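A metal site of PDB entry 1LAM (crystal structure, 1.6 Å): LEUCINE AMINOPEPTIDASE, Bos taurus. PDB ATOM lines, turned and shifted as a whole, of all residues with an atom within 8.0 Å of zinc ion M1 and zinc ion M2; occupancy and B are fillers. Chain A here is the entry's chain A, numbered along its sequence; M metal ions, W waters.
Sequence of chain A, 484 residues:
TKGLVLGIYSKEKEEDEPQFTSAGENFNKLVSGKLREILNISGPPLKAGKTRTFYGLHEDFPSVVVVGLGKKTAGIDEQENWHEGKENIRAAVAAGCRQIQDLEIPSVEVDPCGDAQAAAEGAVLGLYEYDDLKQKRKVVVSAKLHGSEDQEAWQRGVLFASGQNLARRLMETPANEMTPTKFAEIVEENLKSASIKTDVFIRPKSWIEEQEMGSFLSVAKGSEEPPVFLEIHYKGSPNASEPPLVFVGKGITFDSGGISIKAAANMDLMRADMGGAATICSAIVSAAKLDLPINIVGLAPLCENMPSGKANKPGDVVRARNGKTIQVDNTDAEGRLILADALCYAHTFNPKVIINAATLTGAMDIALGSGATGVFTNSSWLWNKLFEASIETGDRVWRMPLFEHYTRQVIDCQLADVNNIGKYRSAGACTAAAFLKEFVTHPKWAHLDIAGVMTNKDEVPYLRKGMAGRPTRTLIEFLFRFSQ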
ATOM      1  N   VAL A 219      10.599  23.441  31.758  1.00  0.00           N
ATOM      2  CA  VAL A 219      10.624  23.084  30.351  1.00  0.00           C
ATOM      3  C   VAL A 219      11.980  23.436  29.736  1.00  0.00           C
ATOM      4  O   VAL A 219      12.598  22.614  29.055  1.00  0.00           O
ATOM      5  CB  VAL A 219       9.525  23.836  29.576  1.00  0.00           C
ATOM      6  CG1 VAL A 219       9.639  23.558  28.082  1.00  0.00           C
ATOM      7  CG2 VAL A 219       8.152  23.424  30.087  1.00  0.00           C
ATOM      8  N   LYS A 250       2.966  31.414  23.072  1.00  0.00           N
ATOM      9  CA  LYS A 250       3.827  30.264  23.357  1.00  0.00           C
ATOM     10  C   LYS A 250       5.041  30.325  22.420  1.00  0.00           C
ATOM     11  O   LYS A 250       4.880  30.270  21.186  1.00  0.00           O
ATOM     12  CB  LYS A 250       3.049  28.963  23.102  1.00  0.00           C
ATOM     13  CG  LYS A 250       3.907  27.695  23.148  1.00  0.00           C
ATOM     14  CD  LYS A 250       3.101  26.458  22.761  1.00  0.00           C
ATOM     15  CE  LYS A 250       4.029  25.251  22.563  1.00  0.00           C
ATOM     16  NZ  LYS A 250       3.305  24.004  22.168  1.00  0.00           N
ATOM     17  N   GLY A 251       6.234  30.442  22.999  1.00  0.00           N
ATOM     18  CA  GLY A 251       7.456  30.513  22.201  1.00  0.00           C
ATOM     19  C   GLY A 251       8.424  29.346  22.306  1.00  0.00           C
ATOM     20  O   GLY A 251       9.593  29.520  22.686  1.00  0.00           O
ATOM     21  N   ILE A 252       7.971  28.135  22.001  1.00  0.00           N
ATOM     22  CA  ILE A 252       8.849  26.975  22.035  1.00  0.00           C
ATOM     23  C   ILE A 252       9.542  26.998  20.657  1.00  0.00           C
ATOM     24  O   ILE A 252       8.930  26.675  19.637  1.00  0.00           O
ATOM     25  CB  ILE A 252       8.041  25.672  22.256  1.00  0.00           C
ATOM     26  CG1 ILE A 252       7.411  25.673  23.663  1.00  0.00           C
ATOM     27  CG2 ILE A 252       8.946  24.444  22.076  1.00  0.00           C
ATOM     28  CD1 ILE A 252       8.421  25.576  24.828  1.00  0.00           C
ATOM     29  N   THR A 253      10.806  27.419  20.622  1.00  0.00           N
ATOM     30  CA  THR A 253      11.541  27.535  19.356  1.00  0.00           C
ATOM     31  C   THR A 253      11.757  26.201  18.635  1.00  0.00           C
ATOM     32  O   THR A 253      11.944  26.161  17.411  1.00  0.00           O
ATOM     33  CB  THR A 253      12.835  28.371  19.526  1.00  0.00           C
ATOM     34  OG1 THR A 253      13.665  27.784  20.533  1.00  0.00           O
ATOM     35  CG2 THR A 253      12.482  29.791  19.965  1.00  0.00           C
ATOM     36  N   PHE A 254      11.801  25.124  19.415  1.00  0.00           N
ATOM     37  CA  PHE A 254      11.854  23.761  18.884  1.00  0.00           C
ATOM     38  C   PHE A 254      11.326  22.804  19.946  1.00  0.00           C
ATOM     39  O   PHE A 254      11.744  22.855  21.109  1.00  0.00           O
ATOM     40  CB  PHE A 254      13.212  23.252  18.389  1.00  0.00           C
ATOM     41  CG  PHE A 254      13.090  21.912  17.675  1.00  0.00           C
ATOM     42  CD1 PHE A 254      12.579  21.871  16.374  1.00  0.00           C
ATOM     43  CD2 PHE A 254      13.308  20.712  18.349  1.00  0.00           C
ATOM     44  CE1 PHE A 254      12.299  20.641  15.755  1.00  0.00           C
ATOM     45  CE2 PHE A 254      13.035  19.488  17.735  1.00  0.00           C
ATOM     46  CZ  PHE A 254      12.514  19.451  16.444  1.00  0.00           C
ATOM     47  N   ASP A 255      10.406  21.956  19.520  1.00  0.00           N
ATOM     48  CA  ASP A 255       9.782  20.983  20.412  1.00  0.00           C
ATOM     49  C   ASP A 255      10.073  19.539  19.944  1.00  0.00           C
ATOM     50  O   ASP A 255       9.503  19.081  18.936  1.00  0.00           O
ATOM     51  CB  ASP A 255       8.267  21.237  20.448  1.00  0.00           C
ATOM     52  CG  ASP A 255       7.550  20.410  21.491  1.00  0.00           C
ATOM     53  OD1 ASP A 255       8.224  19.795  22.348  1.00  0.00           O
ATOM     54  OD2 ASP A 255       6.297  20.379  21.440  1.00  0.00           O
ATOM     55  N   SER A 256      10.950  18.841  20.664  1.00  0.00           N
ATOM     56  CA  SER A 256      11.261  17.443  20.362  1.00  0.00           C
ATOM     57  C   SER A 256      10.304  16.538  21.155  1.00  0.00           C
ATOM     58  O   SER A 256      10.263  15.310  20.959  1.00  0.00           O
ATOM     59  CB  SER A 256      12.687  17.098  20.807  1.00  0.00           C
ATOM     60  OG  SER A 256      12.750  17.047  22.227  1.00  0.00           O
ATOM     61  N   GLY A 257       9.573  17.162  22.074  1.00  0.00           N
ATOM     62  CA  GLY A 257       8.657  16.456  22.937  1.00  0.00           C
ATOM     63  C   GLY A 257       9.308  16.219  24.301  1.00  0.00           C
ATOM     64  O   GLY A 257       8.612  16.074  25.304  1.00  0.00           O
ATOM     65  N   GLY A 258      10.648  16.257  24.338  1.00  0.00           N
ATOM     66  CA  GLY A 258      11.385  16.008  25.573  1.00  0.00           C
ATOM     67  C   GLY A 258      11.497  14.514  25.825  1.00  0.00           C
ATOM     68  O   GLY A 258      11.595  13.734  24.875  1.00  0.00           O
ATOM     69  N   SER A 260       9.202  12.564  26.728  1.00  0.00           N
ATOM     70  CA  SER A 260       8.011  11.999  26.076  1.00  0.00           C
ATOM     71  C   SER A 260       8.249  12.379  24.613  1.00  0.00           C
ATOM     72  O   SER A 260       7.451  13.110  23.997  1.00  0.00           O
ATOM     73  CB  SER A 260       6.766  12.718  26.602  1.00  0.00           C
ATOM     74  OG  SER A 260       6.610  12.552  27.999  1.00  0.00           O
ATOM     75  N   LYS A 262       8.850  12.884  20.590  1.00  0.00           N
ATOM     76  CA  LYS A 262       7.995  12.799  19.403  1.00  0.00           C
ATOM     77  C   LYS A 262       8.498  11.773  18.384  1.00  0.00           C
ATOM     78  O   LYS A 262       9.649  11.344  18.433  1.00  0.00           O
ATOM     79  CB  LYS A 262       7.922  14.159  18.699  1.00  0.00           C
ATOM     80  CG  LYS A 262       7.191  15.220  19.466  1.00  0.00           C
ATOM     81  CD  LYS A 262       7.230  16.548  18.688  1.00  0.00           C
ATOM     82  CE  LYS A 262       6.415  17.623  19.366  1.00  0.00           C
ATOM     83  NZ  LYS A 262       4.982  17.240  19.469  1.00  0.00           N
ATOM     84  N   MET A 270       8.201  21.287  13.882  1.00  0.00           N
ATOM     85  CA  MET A 270       8.166  21.767  15.261  1.00  0.00           C
ATOM     86  C   MET A 270       9.054  23.005  15.486  1.00  0.00           C
ATOM     87  O   MET A 270       9.112  23.553  16.597  1.00  0.00           O
ATOM     88  CB  MET A 270       8.479  20.639  16.245  1.00  0.00           C
ATOM     89  CG  MET A 270       7.398  19.563  16.297  1.00  0.00           C
ATOM     90  SD  MET A 270       5.762  20.274  16.757  1.00  0.00           S
ATOM     91  CE  MET A 270       4.977  20.322  15.208  1.00  0.00           C
ATOM     92  N   ALA A 272       8.300  25.499  14.240  1.00  0.00           N
ATOM     93  CA  ALA A 272       7.239  26.503  14.271  1.00  0.00           C
ATOM     94  C   ALA A 272       6.384  26.419  15.530  1.00  0.00           C
ATOM     95  O   ALA A 272       5.300  27.015  15.570  1.00  0.00           O
ATOM     96  CB  ALA A 272       6.363  26.406  13.018  1.00  0.00           C
ATOM     97  N   ASP A 273       6.880  25.725  16.555  1.00  0.00           N
ATOM     98  CA  ASP A 273       6.117  25.600  17.809  1.00  0.00           C
ATOM     99  C   ASP A 273       6.154  26.931  18.580  1.00  0.00           C
ATOM    100  O   ASP A 273       5.687  27.019  19.716  1.00  0.00           O
ATOM    101  CB  ASP A 273       6.649  24.440  18.657  1.00  0.00           C
ATOM    102  CG  ASP A 273       5.576  23.835  19.579  1.00  0.00           C
ATOM    103  OD1 ASP A 273       4.362  23.866  19.263  1.00  0.00           O
ATOM    104  OD2 ASP A 273       5.966  23.284  20.640  1.00  0.00           O
ATOM    105  N   MET A 274       6.761  27.951  17.964  1.00  0.00           N
ATOM    106  CA  MET A 274       6.818  29.286  18.533  1.00  0.00           C
ATOM    107  C   MET A 274       5.862  30.196  17.736  1.00  0.00           C
ATOM    108  O   MET A 274       5.945  31.426  17.836  1.00  0.00           O
ATOM    109  CB  MET A 274       8.265  29.831  18.522  1.00  0.00           C
ATOM    110  CG  MET A 274       9.130  29.427  17.301  1.00  0.00           C
ATOM    111  SD  MET A 274       8.466  29.916  15.697  1.00  0.00           S
ATOM    112  CE  MET A 274       8.664  31.696  15.777  1.00  0.00           C
ATOM    113  N   ASN A 305      12.431  22.553  23.957  1.00  0.00           N
ATOM    114  CA  ASN A 305      11.978  21.403  24.746  1.00  0.00           C
ATOM    115  C   ASN A 305      12.814  20.245  24.190  1.00  0.00           C
ATOM    116  O   ASN A 305      12.505  19.694  23.127  1.00  0.00           O
ATOM    117  CB  ASN A 305      10.466  21.140  24.565  1.00  0.00           C
ATOM    118  CG  ASN A 305       9.910  20.138  25.568  1.00  0.00           C
ATOM    119  OD1 ASN A 305      10.469  19.959  26.656  1.00  0.00           O
ATOM    120  ND2 ASN A 305       8.812  19.488  25.228  1.00  0.00           N
ATOM    121  N   ASN A 330       3.199  14.240  30.898  1.00  0.00           N
ATOM    122  CA  ASN A 330       3.722  14.109  29.534  1.00  0.00           C
ATOM    123  C   ASN A 330       4.516  15.392  29.246  1.00  0.00           C
ATOM    124  O   ASN A 330       3.954  16.486  29.240  1.00  0.00           O
ATOM    125  CB  ASN A 330       2.557  13.924  28.554  1.00  0.00           C
ATOM    126  CG  ASN A 330       3.026  13.661  27.149  1.00  0.00           C
ATOM    127  OD1 ASN A 330       3.785  14.450  26.605  1.00  0.00           O
ATOM    128  ND2 ASN A 330       2.626  12.537  26.571  1.00  0.00           N
ATOM    129  N   THR A 331       5.834  15.258  29.052  1.00  0.00           N
ATOM    130  CA  THR A 331       6.705  16.407  28.811  1.00  0.00           C
ATOM    131  C   THR A 331       6.478  17.122  27.472  1.00  0.00           C
ATOM    132  O   THR A 331       7.062  18.190  27.229  1.00  0.00           O
ATOM    133  CB  THR A 331       8.204  16.038  28.952  1.00  0.00           C
ATOM    134  OG1 THR A 331       8.586  15.149  27.883  1.00  0.00           O
ATOM    135  CG2 THR A 331       8.471  15.330  30.284  1.00  0.00           C
ATOM    136  N   ASP A 332       5.685  16.511  26.593  1.00  0.00           N
ATOM    137  CA  ASP A 332       5.378  17.093  25.304  1.00  0.00           C
ATOM    138  C   ASP A 332       4.177  18.053  25.439  1.00  0.00           C
ATOM    139  O   ASP A 332       3.832  18.750  24.487  1.00  0.00           O
ATOM    140  CB  ASP A 332       5.126  15.990  24.262  1.00  0.00           C
ATOM    141  CG  ASP A 332       5.140  16.522  22.809  1.00  0.00           C
ATOM    142  OD1 ASP A 332       5.517  17.706  22.548  1.00  0.00           O
ATOM    143  OD2 ASP A 332       4.780  15.724  21.922  1.00  0.00           O
ATOM    144  N   ALA A 333       3.528  18.067  26.601  1.00  0.00           N
ATOM    145  CA  ALA A 333       2.418  19.005  26.847  1.00  0.00           C
ATOM    146  C   ALA A 333       3.093  20.176  27.588  1.00  0.00           C
ATOM    147  O   ALA A 333       2.713  20.531  28.721  1.00  0.00           O
ATOM    148  CB  ALA A 333       1.334  18.355  27.706  1.00  0.00           C
ATOM    149  N   GLU A 334       4.138  20.714  26.966  1.00  0.00           N
ATOM    150  CA  GLU A 334       4.951  21.788  27.554  1.00  0.00           C
ATOM    151  C   GLU A 334       4.477  23.217  27.314  1.00  0.00           C
ATOM    152  O   GLU A 334       4.780  24.116  28.116  1.00  0.00           O
ATOM    153  CB  GLU A 334       6.433  21.650  27.114  1.00  0.00           C
ATOM    154  CG  GLU A 334       6.821  22.352  25.799  1.00  0.00           C
ATOM    155  CD  GLU A 334       6.136  21.787  24.561  1.00  0.00           C
ATOM    156  OE1 GLU A 334       5.949  20.549  24.480  1.00  0.00           O
ATOM    157  OE2 GLU A 334       5.796  22.578  23.642  1.00  0.00           O
ATOM    158  N   GLY A 335       3.736  23.427  26.231  1.00  0.00           N
ATOM    159  CA  GLY A 335       3.255  24.762  25.936  1.00  0.00           C
ATOM    160  C   GLY A 335       2.391  25.288  27.065  1.00  0.00           C
ATOM    161  O   GLY A 335       2.558  26.450  27.491  1.00  0.00           O
ATOM    162  N   ARG A 336       1.512  24.440  27.583  1.00  0.00           N
ATOM    163  CA  ARG A 336       0.628  24.849  28.666  1.00  0.00           C
ATOM    164  C   ARG A 336       1.415  25.145  29.946  1.00  0.00           C
ATOM    165  O   ARG A 336       1.029  26.008  30.750  1.00  0.00           O
ATOM    166  CB  ARG A 336      -0.520  23.837  28.884  1.00  0.00           C
ATOM    167  CG  ARG A 336      -0.120  22.483  29.456  1.00  0.00           C
ATOM    168  CD  ARG A 336      -1.233  21.462  29.229  1.00  0.00           C
ATOM    169  NE  ARG A 336      -1.252  20.990  27.835  1.00  0.00           N
ATOM    170  CZ  ARG A 336      -2.071  20.060  27.349  1.00  0.00           C
ATOM    171  NH1 ARG A 336      -2.990  19.487  28.112  1.00  0.00           N
ATOM    172  NH2 ARG A 336      -1.983  19.708  26.065  1.00  0.00           N
ATOM    173  N   ILE A 338       4.605  26.558  30.110  1.00  0.00           N
ATOM    174  CA  ILE A 338       5.199  27.885  30.003  1.00  0.00           C
ATOM    175  C   ILE A 338       4.109  28.986  29.979  1.00  0.00           C
ATOM    176  O   ILE A 338       4.335  30.101  30.485  1.00  0.00           O
ATOM    177  CB  ILE A 338       6.188  28.026  28.774  1.00  0.00           C
ATOM    178  CG1 ILE A 338       5.438  28.231  27.455  1.00  0.00           C
ATOM    179  CG2 ILE A 338       7.114  26.783  28.696  1.00  0.00           C
ATOM    180  CD1 ILE A 338       6.373  28.480  26.267  1.00  0.00           C
ATOM    181  N   ALA A 358      -1.253  29.978  20.732  1.00  0.00           N
ATOM    182  CA  ALA A 358      -0.328  28.864  20.863  1.00  0.00           C
ATOM    183  C   ALA A 358      -0.590  27.738  19.865  1.00  0.00           C
ATOM    184  O   ALA A 358      -1.749  27.423  19.584  1.00  0.00           O
ATOM    185  CB  ALA A 358      -0.426  28.291  22.275  1.00  0.00           C
ATOM    186  N   THR A 359       0.486  27.140  19.346  1.00  0.00           N
ATOM    187  CA  THR A 359       0.392  25.977  18.447  1.00  0.00           C
ATOM    188  C   THR A 359       0.345  24.910  19.531  1.00  0.00           C
ATOM    189  O   THR A 359       1.310  24.172  19.758  1.00  0.00           O
ATOM    190  CB  THR A 359       1.672  25.829  17.582  1.00  0.00           C
ATOM    191  OG1 THR A 359       2.834  25.970  18.392  1.00  0.00           O
ATOM    192  CG2 THR A 359       1.716  26.871  16.466  1.00  0.00           C
ATOM    193  N   LEU A 360      -0.800  24.818  20.204  1.00  0.00           N
ATOM    194  CA  LEU A 360      -0.924  23.930  21.346  1.00  0.00           C
ATOM    195  C   LEU A 360      -1.182  22.440  21.222  1.00  0.00           C
ATOM    196  O   LEU A 360      -0.464  21.643  21.845  1.00  0.00           O
ATOM    197  CB  LEU A 360      -1.877  24.559  22.370  1.00  0.00           C
ATOM    198  CG  LEU A 360      -1.654  24.219  23.857  1.00  0.00           C
ATOM    199  CD1 LEU A 360      -0.318  24.771  24.353  1.00  0.00           C
ATOM    200  CD2 LEU A 360      -2.796  24.782  24.696  1.00  0.00           C
ATOM    201  N   THR A 361      -2.178  22.020  20.429  1.00  0.00           N
ATOM    202  CA  THR A 361      -2.479  20.593  20.390  1.00  0.00           C
ATOM    203  C   THR A 361      -2.709  19.970  19.030  1.00  0.00           C
ATOM    204  O   THR A 361      -3.271  20.602  18.127  1.00  0.00           O
ATOM    205  CB  THR A 361      -3.751  20.268  21.252  1.00  0.00           C
ATOM    206  OG1 THR A 361      -4.914  20.866  20.647  1.00  0.00           O
ATOM    207  CG2 THR A 361      -3.604  20.791  22.694  1.00  0.00           C
HETATM  208 ZN    ZN M   1       5.036  19.581  22.954  1.00  0.00          ZN
HETATM  209 ZN    ZN M   2       4.747  22.405  21.930  1.00  0.00          ZN
HETATM  210  O   HOH W   1       3.637  20.824  22.201  1.00  0.00           O
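The backbone NH (N) of Asp 332 lies within hydrogen-bond range of the backbone carbonyl oxygen (O) of Gly 257 (3.2 Å).
OD1 of Asn 330 lies within hydrogen-bond range of N of Asp 332, at 2.8 Å.
OD1 of Asp 273 is in hydrogen-bond range of OG1 of Thr 359, 2.7 Å away.
The backbone NH (N) of Ile 252 lies within hydrogen-bond range of the backbone carbonyl oxygen (O) of Asp 273, 3.4 Å away.
The side-chain amide nitrogen (ND2) of Asn 305 lies close to the side-chain carboxylate (OE1) of Glu 334, at 3.1 Å.
The side-chain carboxylate of Asp 255 is in hydrogen-bond range of the side-chain amide nitrogen of Asn 305, at 3.0 Å.
The side-chain carboxylate (OD1) of Asp 255 sits at hydrogen-bond distance from the backbone NH (N) of Gly 257 (3.0 Å).
NZ of Lys 250 lies close to O of Thr 359 (3.1 Å).
Within 4 Å of zinc ion M1: Asp 255, Asp 332 and Glu 334.
The nearest printed residue that does not touch zinc ion M1 is Lys 262 (4.2 Å).
Of the 29 residues printed, 4 come within 4 Å of zinc ion M2.
Along chain A the residues within 4 Å of zinc ion M2 span positions 250 to 334.
The nearest printed residue that does not touch zinc ion M2 is Thr 359 (4.4 Å).
Zinc ion M1 is bound by OD1 of Asp 332 (2.0 Å).
Water W1 binds zinc ion M1, 2.0 Å away.
OE1 of Glu 334 binds zinc ion M1, at 2.0 Å.
O of Asp 332 binds zinc ion M1 (2.1 Å).
OD2 of Asp 255 binds zinc ion M1, at 2.1 Å.
Zinc ion M1 has five donor atoms within binding distance.
Zinc ion M2 is bound by water W1 (2.0 Å).
OD2 of Asp 273 binds zinc ion M2 (2.0 Å).
OE2 of Glu 334 binds zinc ion M2.
The side-chain amino group (NZ) of Lys 250 is bound to zinc ion M2 (2.2 Å).
Zinc ion M2 is bound by OD2 of Asp 255.
Zinc ion M2 has five donor atoms within binding distance.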
